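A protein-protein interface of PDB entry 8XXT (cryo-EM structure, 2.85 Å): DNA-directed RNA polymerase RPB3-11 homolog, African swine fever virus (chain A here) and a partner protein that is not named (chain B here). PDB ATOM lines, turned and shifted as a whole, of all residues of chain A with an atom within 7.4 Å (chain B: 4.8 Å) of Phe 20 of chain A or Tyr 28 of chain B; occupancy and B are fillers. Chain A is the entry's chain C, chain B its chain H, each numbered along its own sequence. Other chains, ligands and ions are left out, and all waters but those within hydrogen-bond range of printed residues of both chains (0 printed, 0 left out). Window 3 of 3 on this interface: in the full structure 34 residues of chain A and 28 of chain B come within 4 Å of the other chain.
Of chain B, only Ala 24 (3.95 Å), Glu 27 (3.9 Å), Tyr 28 (3.4 Å) and Leu 54 (3.7 Å) come within 4 Å of Phe 20 of chain A. Tyr 28 of chain B touches just one residue of chain A: Phe 20 (3.4 Å). Of the printed residues of chain B, Ala 24 of chain A touches Ala 24 (3.9 Å). Printed residues of chain A within 4 Å of Leu 54 of chain B: Asn 18 (3.1 Å), Phe 20 (3.7 Å) and Ile 21 (3.8 Å). Of the printed residues of chain B, Asn 23 of chain A touches Glu 27. Printed residues of chain A within 4 Å of Ala 24 of chain B: Phe 20, Ile 21 and Ala 24. Asp 15 of chain A touches none of the printed residues of chain B. The nearest residue of chain B that does not touch Phe 20 of chain A is Thr 31 of chain B (4.2 Å). The nearest printed residue of chain A that does not touch Ala 24 of chain B is Asn 18 of chain A (6.4 Å).
The backbone carbonyl oxygen of Leu 19 of chain A is in hydrogen-bond range of the side-chain amide nitrogen of Asn 23 of chain A, at 2.8 Å. O of Tyr 28 of chain B is in hydrogen-bond range of OG1 of Thr 31 of chain B.
Printed residues of chain A that touch a printed residue of chain B: Asn 18, Phe 20, Ile 21, Asn 23 and Ala 24. Hydrophobic or aromatic side chains of chain A that line the printed part of chain B: Phe 20, Ile 21 and Ala 24. Among the printed residues, no Asp or Glu carboxylate lies within 4 Å of a Lys or Arg side-chain nitrogen of the other chain.
Among the printed residues, pairs that only touch across the chains: Asn 18 of chain A with Leu 54 of chain B (3.1 Å), Phe 20 of chain A with Ala 24 of chain B (3.95 Å), Phe 20 of chain A with Glu 27 of chain B (3.9 Å), Phe 20 of chain A with Tyr 28 of chain B (3.4 Å), Phe 20 of chain A with Leu 54 of chain B (3.7 Å), Ile 21 of chain A with Ala 24 of chain B (3.7 Å), Ile 21 of chain A with Leu 54 of chain B (3.8 Å), Asn 23 of chain A with Glu 27 of chain B (3.9 Å) and Ala 24 of chain A with Ala 24 of chain B (3.9 Å).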
ATOM      1  N   ASP A  15     -22.864   1.265  12.390  1.00  0.00           N
ATOM      2  CA  ASP A  15     -22.218   1.821  13.578  1.00  0.00           C
ATOM      3  C   ASP A  15     -20.721   1.573  13.463  1.00  0.00           C
ATOM      4  O   ASP A  15     -20.211   0.520  13.846  1.00  0.00           O
ATOM      5  CB  ASP A  15     -22.794   1.199  14.842  1.00  0.00           C
ATOM      6  CG  ASP A  15     -22.247   1.827  16.099  1.00  0.00           C
ATOM      7  OD1 ASP A  15     -21.772   2.978  16.031  1.00  0.00           O
ATOM      8  OD2 ASP A  15     -22.285   1.168  17.157  1.00  0.00           O
ATOM      9  N   PHE A  16     -20.002   2.566  12.936  1.00  0.00           N
ATOM     10  CA  PHE A  16     -18.560   2.446  12.770  1.00  0.00           C
ATOM     11  C   PHE A  16     -17.807   2.489  14.091  1.00  0.00           C
ATOM     12  O   PHE A  16     -16.599   2.238  14.099  1.00  0.00           O
ATOM     13  CB  PHE A  16     -18.046   3.546  11.844  1.00  0.00           C
ATOM     14  CG  PHE A  16     -18.339   3.300  10.394  1.00  0.00           C
ATOM     15  CD1 PHE A  16     -17.778   2.223   9.736  1.00  0.00           C
ATOM     16  CD2 PHE A  16     -19.172   4.148   9.687  1.00  0.00           C
ATOM     17  CE1 PHE A  16     -18.043   1.995   8.403  1.00  0.00           C
ATOM     18  CE2 PHE A  16     -19.440   3.922   8.353  1.00  0.00           C
ATOM     19  CZ  PHE A  16     -18.874   2.844   7.712  1.00  0.00           C
ATOM     20  N   SER A  17     -18.482   2.802  15.200  1.00  0.00           N
ATOM     21  CA  SER A  17     -17.829   2.776  16.503  1.00  0.00           C
ATOM     22  C   SER A  17     -17.255   1.402  16.819  1.00  0.00           C
ATOM     23  O   SER A  17     -16.237   1.301  17.512  1.00  0.00           O
ATOM     24  CB  SER A  17     -18.814   3.195  17.593  1.00  0.00           C
ATOM     25  OG  SER A  17     -18.250   3.022  18.881  1.00  0.00           O
ATOM     26  N   ASN A  18     -17.893   0.340  16.336  1.00  0.00           N
ATOM     27  CA  ASN A  18     -17.347  -0.999  16.495  1.00  0.00           C
ATOM     28  C   ASN A  18     -16.071  -1.122  15.673  1.00  0.00           C
ATOM     29  O   ASN A  18     -16.080  -0.872  14.463  1.00  0.00           O
ATOM     30  CB  ASN A  18     -18.371  -2.043  16.063  1.00  0.00           C
ATOM     31  CG  ASN A  18     -18.336  -3.284  16.926  1.00  0.00           C
ATOM     32  OD1 ASN A  18     -17.958  -4.358  16.470  1.00  0.00           O
ATOM     33  ND2 ASN A  18     -18.736  -3.142  18.181  1.00  0.00           N
ATOM     34  N   LEU A  19     -14.976  -1.504  16.331  1.00  0.00           N
ATOM     35  CA  LEU A  19     -13.682  -1.533  15.659  1.00  0.00           C
ATOM     36  C   LEU A  19     -13.675  -2.530  14.511  1.00  0.00           C
ATOM     37  O   LEU A  19     -13.154  -2.238  13.428  1.00  0.00           O
ATOM     38  CB  LEU A  19     -12.580  -1.864  16.664  1.00  0.00           C
ATOM     39  CG  LEU A  19     -12.500  -0.953  17.890  1.00  0.00           C
ATOM     40  CD1 LEU A  19     -11.346  -1.359  18.788  1.00  0.00           C
ATOM     41  CD2 LEU A  19     -12.374   0.500  17.472  1.00  0.00           C
ATOM     42  N   PHE A  20     -14.251  -3.715  14.725  1.00  0.00           N
ATOM     43  CA  PHE A  20     -14.243  -4.739  13.687  1.00  0.00           C
ATOM     44  C   PHE A  20     -15.004  -4.281  12.452  1.00  0.00           C
ATOM     45  O   PHE A  20     -14.563  -4.511  11.322  1.00  0.00           O
ATOM     46  CB  PHE A  20     -14.837  -6.036  14.227  1.00  0.00           C
ATOM     47  CG  PHE A  20     -14.143  -6.553  15.444  1.00  0.00           C
ATOM     48  CD1 PHE A  20     -12.827  -6.967  15.379  1.00  0.00           C
ATOM     49  CD2 PHE A  20     -14.804  -6.621  16.655  1.00  0.00           C
ATOM     50  CE1 PHE A  20     -12.184  -7.442  16.501  1.00  0.00           C
ATOM     51  CE2 PHE A  20     -14.166  -7.094  17.780  1.00  0.00           C
ATOM     52  CZ  PHE A  20     -12.855  -7.508  17.703  1.00  0.00           C
ATOM     53  N   ILE A  21     -16.149  -3.627  12.650  1.00  0.00           N
ATOM     54  CA  ILE A  21     -16.967  -3.203  11.518  1.00  0.00           C
ATOM     55  C   ILE A  21     -16.220  -2.176  10.680  1.00  0.00           C
ATOM     56  O   ILE A  21     -16.164  -2.278   9.449  1.00  0.00           O
ATOM     57  CB  ILE A  21     -18.320  -2.661  12.004  1.00  0.00           C
ATOM     58  CG1 ILE A  21     -19.100  -3.756  12.730  1.00  0.00           C
ATOM     59  CG2 ILE A  21     -19.121  -2.124  10.838  1.00  0.00           C
ATOM     60  CD1 ILE A  21     -19.246  -5.027  11.938  1.00  0.00           C
ATOM     61  N   LYS A  22     -15.628  -1.173  11.333  1.00  0.00           N
ATOM     62  CA  LYS A  22     -14.888  -0.152  10.597  1.00  0.00           C
ATOM     63  C   LYS A  22     -13.671  -0.745   9.902  1.00  0.00           C
ATOM     64  O   LYS A  22     -13.391  -0.417   8.741  1.00  0.00           O
ATOM     65  CB  LYS A  22     -14.468   0.980  11.532  1.00  0.00           C
ATOM     66  CG  LYS A  22     -13.990   2.229  10.803  1.00  0.00           C
ATOM     67  CD  LYS A  22     -13.240   3.172  11.728  1.00  0.00           C
ATOM     68  CE  LYS A  22     -14.149   3.719  12.813  1.00  0.00           C
ATOM     69  NZ  LYS A  22     -13.445   4.664  13.720  1.00  0.00           N
ATOM     70  N   ASN A  23     -12.939  -1.621  10.593  1.00  0.00           N
ATOM     71  CA  ASN A  23     -11.757  -2.230   9.997  1.00  0.00           C
ATOM     72  C   ASN A  23     -12.121  -3.039   8.759  1.00  0.00           C
ATOM     73  O   ASN A  23     -11.483  -2.904   7.711  1.00  0.00           O
ATOM     74  CB  ASN A  23     -11.042  -3.107  11.024  1.00  0.00           C
ATOM     75  CG  ASN A  23     -10.417  -2.300  12.139  1.00  0.00           C
ATOM     76  OD1 ASN A  23      -9.938  -1.187  11.923  1.00  0.00           O
ATOM     77  ND2 ASN A  23     -10.417  -2.858  13.345  1.00  0.00           N
ATOM     78  N   ALA A  24     -13.159  -3.873   8.856  1.00  0.00           N
ATOM     79  CA  ALA A  24     -13.586  -4.654   7.701  1.00  0.00           C
ATOM     80  C   ALA A  24     -14.058  -3.748   6.572  1.00  0.00           C
ATOM     81  O   ALA A  24     -13.709  -3.956   5.404  1.00  0.00           O
ATOM     82  CB  ALA A  24     -14.689  -5.630   8.105  1.00  0.00           C
ATOM     83  N   ALA A  25     -14.850  -2.726   6.905  1.00  0.00           N
ATOM     84  CA  ALA A  25     -15.370  -1.833   5.878  1.00  0.00           C
ATOM     85  C   ALA A  25     -14.239  -1.190   5.090  1.00  0.00           C
ATOM     86  O   ALA A  25     -14.232  -1.222   3.855  1.00  0.00           O
ATOM     87  CB  ALA A  25     -16.261  -0.767   6.511  1.00  0.00           C
ATOM     88  N   LYS A  26     -13.251  -0.629   5.789  1.00  0.00           N
ATOM     89  CA  LYS A  26     -12.165   0.021   5.066  1.00  0.00           C
ATOM     90  C   LYS A  26     -11.251  -0.996   4.398  1.00  0.00           C
ATOM     91  O   LYS A  26     -10.618  -0.679   3.385  1.00  0.00           O
ATOM     92  CB  LYS A  26     -11.357   0.932   5.989  1.00  0.00           C
ATOM     93  CG  LYS A  26     -10.797   0.263   7.223  1.00  0.00           C
ATOM     94  CD  LYS A  26      -9.625   1.053   7.774  1.00  0.00           C
ATOM     95  CE  LYS A  26      -9.715   1.206   9.282  1.00  0.00           C
ATOM     96  NZ  LYS A  26     -10.703   2.250   9.672  1.00  0.00           N
ATOM     97  N   ALA B  24     -15.552  -9.151   9.613  1.00  0.00           N
ATOM     98  CA  ALA B  24     -15.640  -8.709  10.999  1.00  0.00           C
ATOM     99  C   ALA B  24     -15.767  -9.900  11.934  1.00  0.00           C
ATOM    100  O   ALA B  24     -15.102  -9.960  12.974  1.00  0.00           O
ATOM    101  CB  ALA B  24     -16.816  -7.754  11.180  1.00  0.00           C
ATOM    102  N   ARG B  25     -16.595 -10.875  11.564  1.00  0.00           N
ATOM    103  CA  ARG B  25     -16.730 -12.085  12.360  1.00  0.00           C
ATOM    104  C   ARG B  25     -15.422 -12.855  12.409  1.00  0.00           C
ATOM    105  O   ARG B  25     -15.051 -13.373  13.462  1.00  0.00           O
ATOM    106  CB  ARG B  25     -17.849 -12.958  11.795  1.00  0.00           C
ATOM    107  CG  ARG B  25     -17.936 -14.337  12.415  1.00  0.00           C
ATOM    108  CD  ARG B  25     -19.077 -15.132  11.816  1.00  0.00           C
ATOM    109  NE  ARG B  25     -18.928 -15.290  10.376  1.00  0.00           N
ATOM    110  CZ  ARG B  25     -19.870 -15.766   9.575  1.00  0.00           C
ATOM    111  NH1 ARG B  25     -21.045 -16.147  10.044  1.00  0.00           N
ATOM    112  NH2 ARG B  25     -19.627 -15.860   8.272  1.00  0.00           N
ATOM    113  N   THR B  26     -14.710 -12.943  11.284  1.00  0.00           N
ATOM    114  CA  THR B  26     -13.430 -13.650  11.280  1.00  0.00           C
ATOM    115  C   THR B  26     -12.442 -13.007  12.251  1.00  0.00           C
ATOM    116  O   THR B  26     -11.812 -13.692  13.073  1.00  0.00           O
ATOM    117  CB  THR B  26     -12.851 -13.673   9.866  1.00  0.00           C
ATOM    118  OG1 THR B  26     -13.772 -14.319   8.982  1.00  0.00           O
ATOM    119  CG2 THR B  26     -11.536 -14.422   9.842  1.00  0.00           C
ATOM    120  N   GLU B  27     -12.310 -11.681  12.179  1.00  0.00           N
ATOM    121  CA  GLU B  27     -11.432 -10.974  13.103  1.00  0.00           C
ATOM    122  C   GLU B  27     -11.897 -11.134  14.542  1.00  0.00           C
ATOM    123  O   GLU B  27     -11.074 -11.135  15.462  1.00  0.00           O
ATOM    124  CB  GLU B  27     -11.354  -9.497  12.728  1.00  0.00           C
ATOM    125  CG  GLU B  27     -10.853  -9.245  11.315  1.00  0.00           C
ATOM    126  CD  GLU B  27     -10.871  -7.776  10.941  1.00  0.00           C
ATOM    127  OE1 GLU B  27     -10.966  -6.929  11.854  1.00  0.00           O
ATOM    128  OE2 GLU B  27     -10.792  -7.467   9.734  1.00  0.00           O
ATOM    129  N   TYR B  28     -13.205 -11.273  14.759  1.00  0.00           N
ATOM    130  CA  TYR B  28     -13.706 -11.507  16.107  1.00  0.00           C
ATOM    131  C   TYR B  28     -13.401 -12.925  16.585  1.00  0.00           C
ATOM    132  O   TYR B  28     -13.263 -13.153  17.790  1.00  0.00           O
ATOM    133  CB  TYR B  28     -15.204 -11.217  16.154  1.00  0.00           C
ATOM    134  CG  TYR B  28     -15.798 -11.195  17.540  1.00  0.00           C
ATOM    135  CD1 TYR B  28     -15.750 -10.050  18.319  1.00  0.00           C
ATOM    136  CD2 TYR B  28     -16.432 -12.307  18.056  1.00  0.00           C
ATOM    137  CE1 TYR B  28     -16.301 -10.026  19.586  1.00  0.00           C
ATOM    138  CE2 TYR B  28     -16.985 -12.294  19.319  1.00  0.00           C
ATOM    139  CZ  TYR B  28     -16.918 -11.154  20.079  1.00  0.00           C
ATOM    140  OH  TYR B  28     -17.473 -11.147  21.336  1.00  0.00           O
ATOM    141  N   ILE B  29     -13.310 -13.890  15.663  1.00  0.00           N
ATOM    142  CA  ILE B  29     -12.821 -15.221  16.029  1.00  0.00           C
ATOM    143  C   ILE B  29     -11.375 -15.140  16.479  1.00  0.00           C
ATOM    144  O   ILE B  29     -10.997 -15.689  17.519  1.00  0.00           O
ATOM    145  CB  ILE B  29     -12.955 -16.226  14.867  1.00  0.00           C
ATOM    146  CG1 ILE B  29     -14.267 -16.105  14.109  1.00  0.00           C
ATOM    147  CG2 ILE B  29     -12.798 -17.647  15.390  1.00  0.00           C
ATOM    148  CD1 ILE B  29     -15.443 -16.007  14.991  1.00  0.00           C
ATOM    149  N   LYS B  30     -10.543 -14.451  15.696  1.00  0.00           N
ATOM    150  CA  LYS B  30      -9.114 -14.452  15.983  1.00  0.00           C
ATOM    151  C   LYS B  30      -8.799 -13.873  17.356  1.00  0.00           C
ATOM    152  O   LYS B  30      -7.718 -14.135  17.893  1.00  0.00           O
ATOM    153  CB  LYS B  30      -8.358 -13.690  14.897  1.00  0.00           C
ATOM    154  CG  LYS B  30      -8.595 -14.230  13.497  1.00  0.00           C
ATOM    155  CD  LYS B  30      -7.416 -13.955  12.586  1.00  0.00           C
ATOM    156  CE  LYS B  30      -7.722 -12.834  11.611  1.00  0.00           C
ATOM    157  NZ  LYS B  30      -7.711 -11.501  12.274  1.00  0.00           N
ATOM    158  N   THR B  31      -9.716 -13.107  17.941  1.00  0.00           N
ATOM    159  CA  THR B  31      -9.540 -12.575  19.285  1.00  0.00           C
ATOM    160  C   THR B  31     -10.280 -13.376  20.349  1.00  0.00           C
ATOM    161  O   THR B  31     -10.329 -12.940  21.503  1.00  0.00           O
ATOM    162  CB  THR B  31     -10.002 -11.117  19.347  1.00  0.00           C
ATOM    163  OG1 THR B  31     -11.432 -11.068  19.390  1.00  0.00           O
ATOM    164  CG2 THR B  31      -9.508 -10.346  18.139  1.00  0.00           C
ATOM    165  N   LYS B  32     -10.859 -14.523  20.002  1.00  0.00           N
ATOM    166  CA  LYS B  32     -11.597 -15.303  20.989  1.00  0.00           C
ATOM    167  C   LYS B  32     -11.148 -16.759  20.996  1.00  0.00           C
ATOM    168  O   LYS B  32     -11.217 -17.428  22.032  1.00  0.00           O
ATOM    169  CB  LYS B  32     -13.103 -15.200  20.730  1.00  0.00           C
ATOM    170  CG  LYS B  32     -13.970 -16.010  21.686  1.00  0.00           C
ATOM    171  CD  LYS B  32     -13.653 -15.697  23.141  1.00  0.00           C
ATOM    172  CE  LYS B  32     -14.905 -15.695  24.004  1.00  0.00           C
ATOM    173  NZ  LYS B  32     -15.526 -14.346  24.096  1.00  0.00           N
ATOM    174  N   ILE B  49     -18.332 -17.587  20.130  1.00  0.00           N
ATOM    175  CA  ILE B  49     -18.537 -16.157  20.058  1.00  0.00           C
ATOM    176  C   ILE B  49     -19.979 -15.839  20.432  1.00  0.00           C
ATOM    177  O   ILE B  49     -20.831 -16.721  20.557  1.00  0.00           O
ATOM    178  CB  ILE B  49     -18.248 -15.639  18.643  1.00  0.00           C
ATOM    179  CG1 ILE B  49     -18.770 -16.650  17.639  1.00  0.00           C
ATOM    180  CG2 ILE B  49     -16.759 -15.601  18.419  1.00  0.00           C
ATOM    181  CD1 ILE B  49     -18.516 -16.276  16.226  1.00  0.00           C
ATOM    182  N   GLU B  50     -20.250 -14.550  20.627  1.00  0.00           N
ATOM    183  CA  GLU B  50     -21.584 -13.982  20.491  1.00  0.00           C
ATOM    184  C   GLU B  50     -21.486 -12.817  19.519  1.00  0.00           C
ATOM    185  O   GLU B  50     -20.699 -11.891  19.738  1.00  0.00           O
ATOM    186  CB  GLU B  50     -22.153 -13.509  21.830  1.00  0.00           C
ATOM    187  CG  GLU B  50     -21.999 -14.498  22.966  1.00  0.00           C
ATOM    188  CD  GLU B  50     -21.487 -13.846  24.233  1.00  0.00           C
ATOM    189  OE1 GLU B  50     -20.448 -13.155  24.168  1.00  0.00           O
ATOM    190  OE2 GLU B  50     -22.127 -14.021  25.291  1.00  0.00           O
ATOM    191  N   LEU B  51     -22.270 -12.865  18.445  1.00  0.00           N
ATOM    192  CA  LEU B  51     -22.156 -11.900  17.360  1.00  0.00           C
ATOM    193  C   LEU B  51     -23.221 -10.814  17.421  1.00  0.00           C
ATOM    194  O   LEU B  51     -23.415 -10.096  16.436  1.00  0.00           O
ATOM    195  CB  LEU B  51     -22.214 -12.616  16.013  1.00  0.00           C
ATOM    196  CG  LEU B  51     -21.085 -13.610  15.746  1.00  0.00           C
ATOM    197  CD1 LEU B  51     -21.508 -14.620  14.703  1.00  0.00           C
ATOM    198  CD2 LEU B  51     -19.828 -12.893  15.308  1.00  0.00           C
ATOM    199  N   LEU B  54     -21.722  -7.287  16.805  1.00  0.00           N
ATOM    200  CA  LEU B  54     -21.306  -7.090  15.420  1.00  0.00           C
ATOM    201  C   LEU B  54     -22.507  -6.888  14.508  1.00  0.00           C
ATOM    202  O   LEU B  54     -22.470  -6.056  13.593  1.00  0.00           O
ATOM    203  CB  LEU B  54     -20.482  -8.282  14.935  1.00  0.00           C
ATOM    204  CG  LEU B  54     -19.207  -8.661  15.681  1.00  0.00           C
ATOM    205  CD1 LEU B  54     -18.380  -9.599  14.826  1.00  0.00           C
ATOM    206  CD2 LEU B  54     -18.409  -7.434  16.045  1.00  0.00           C
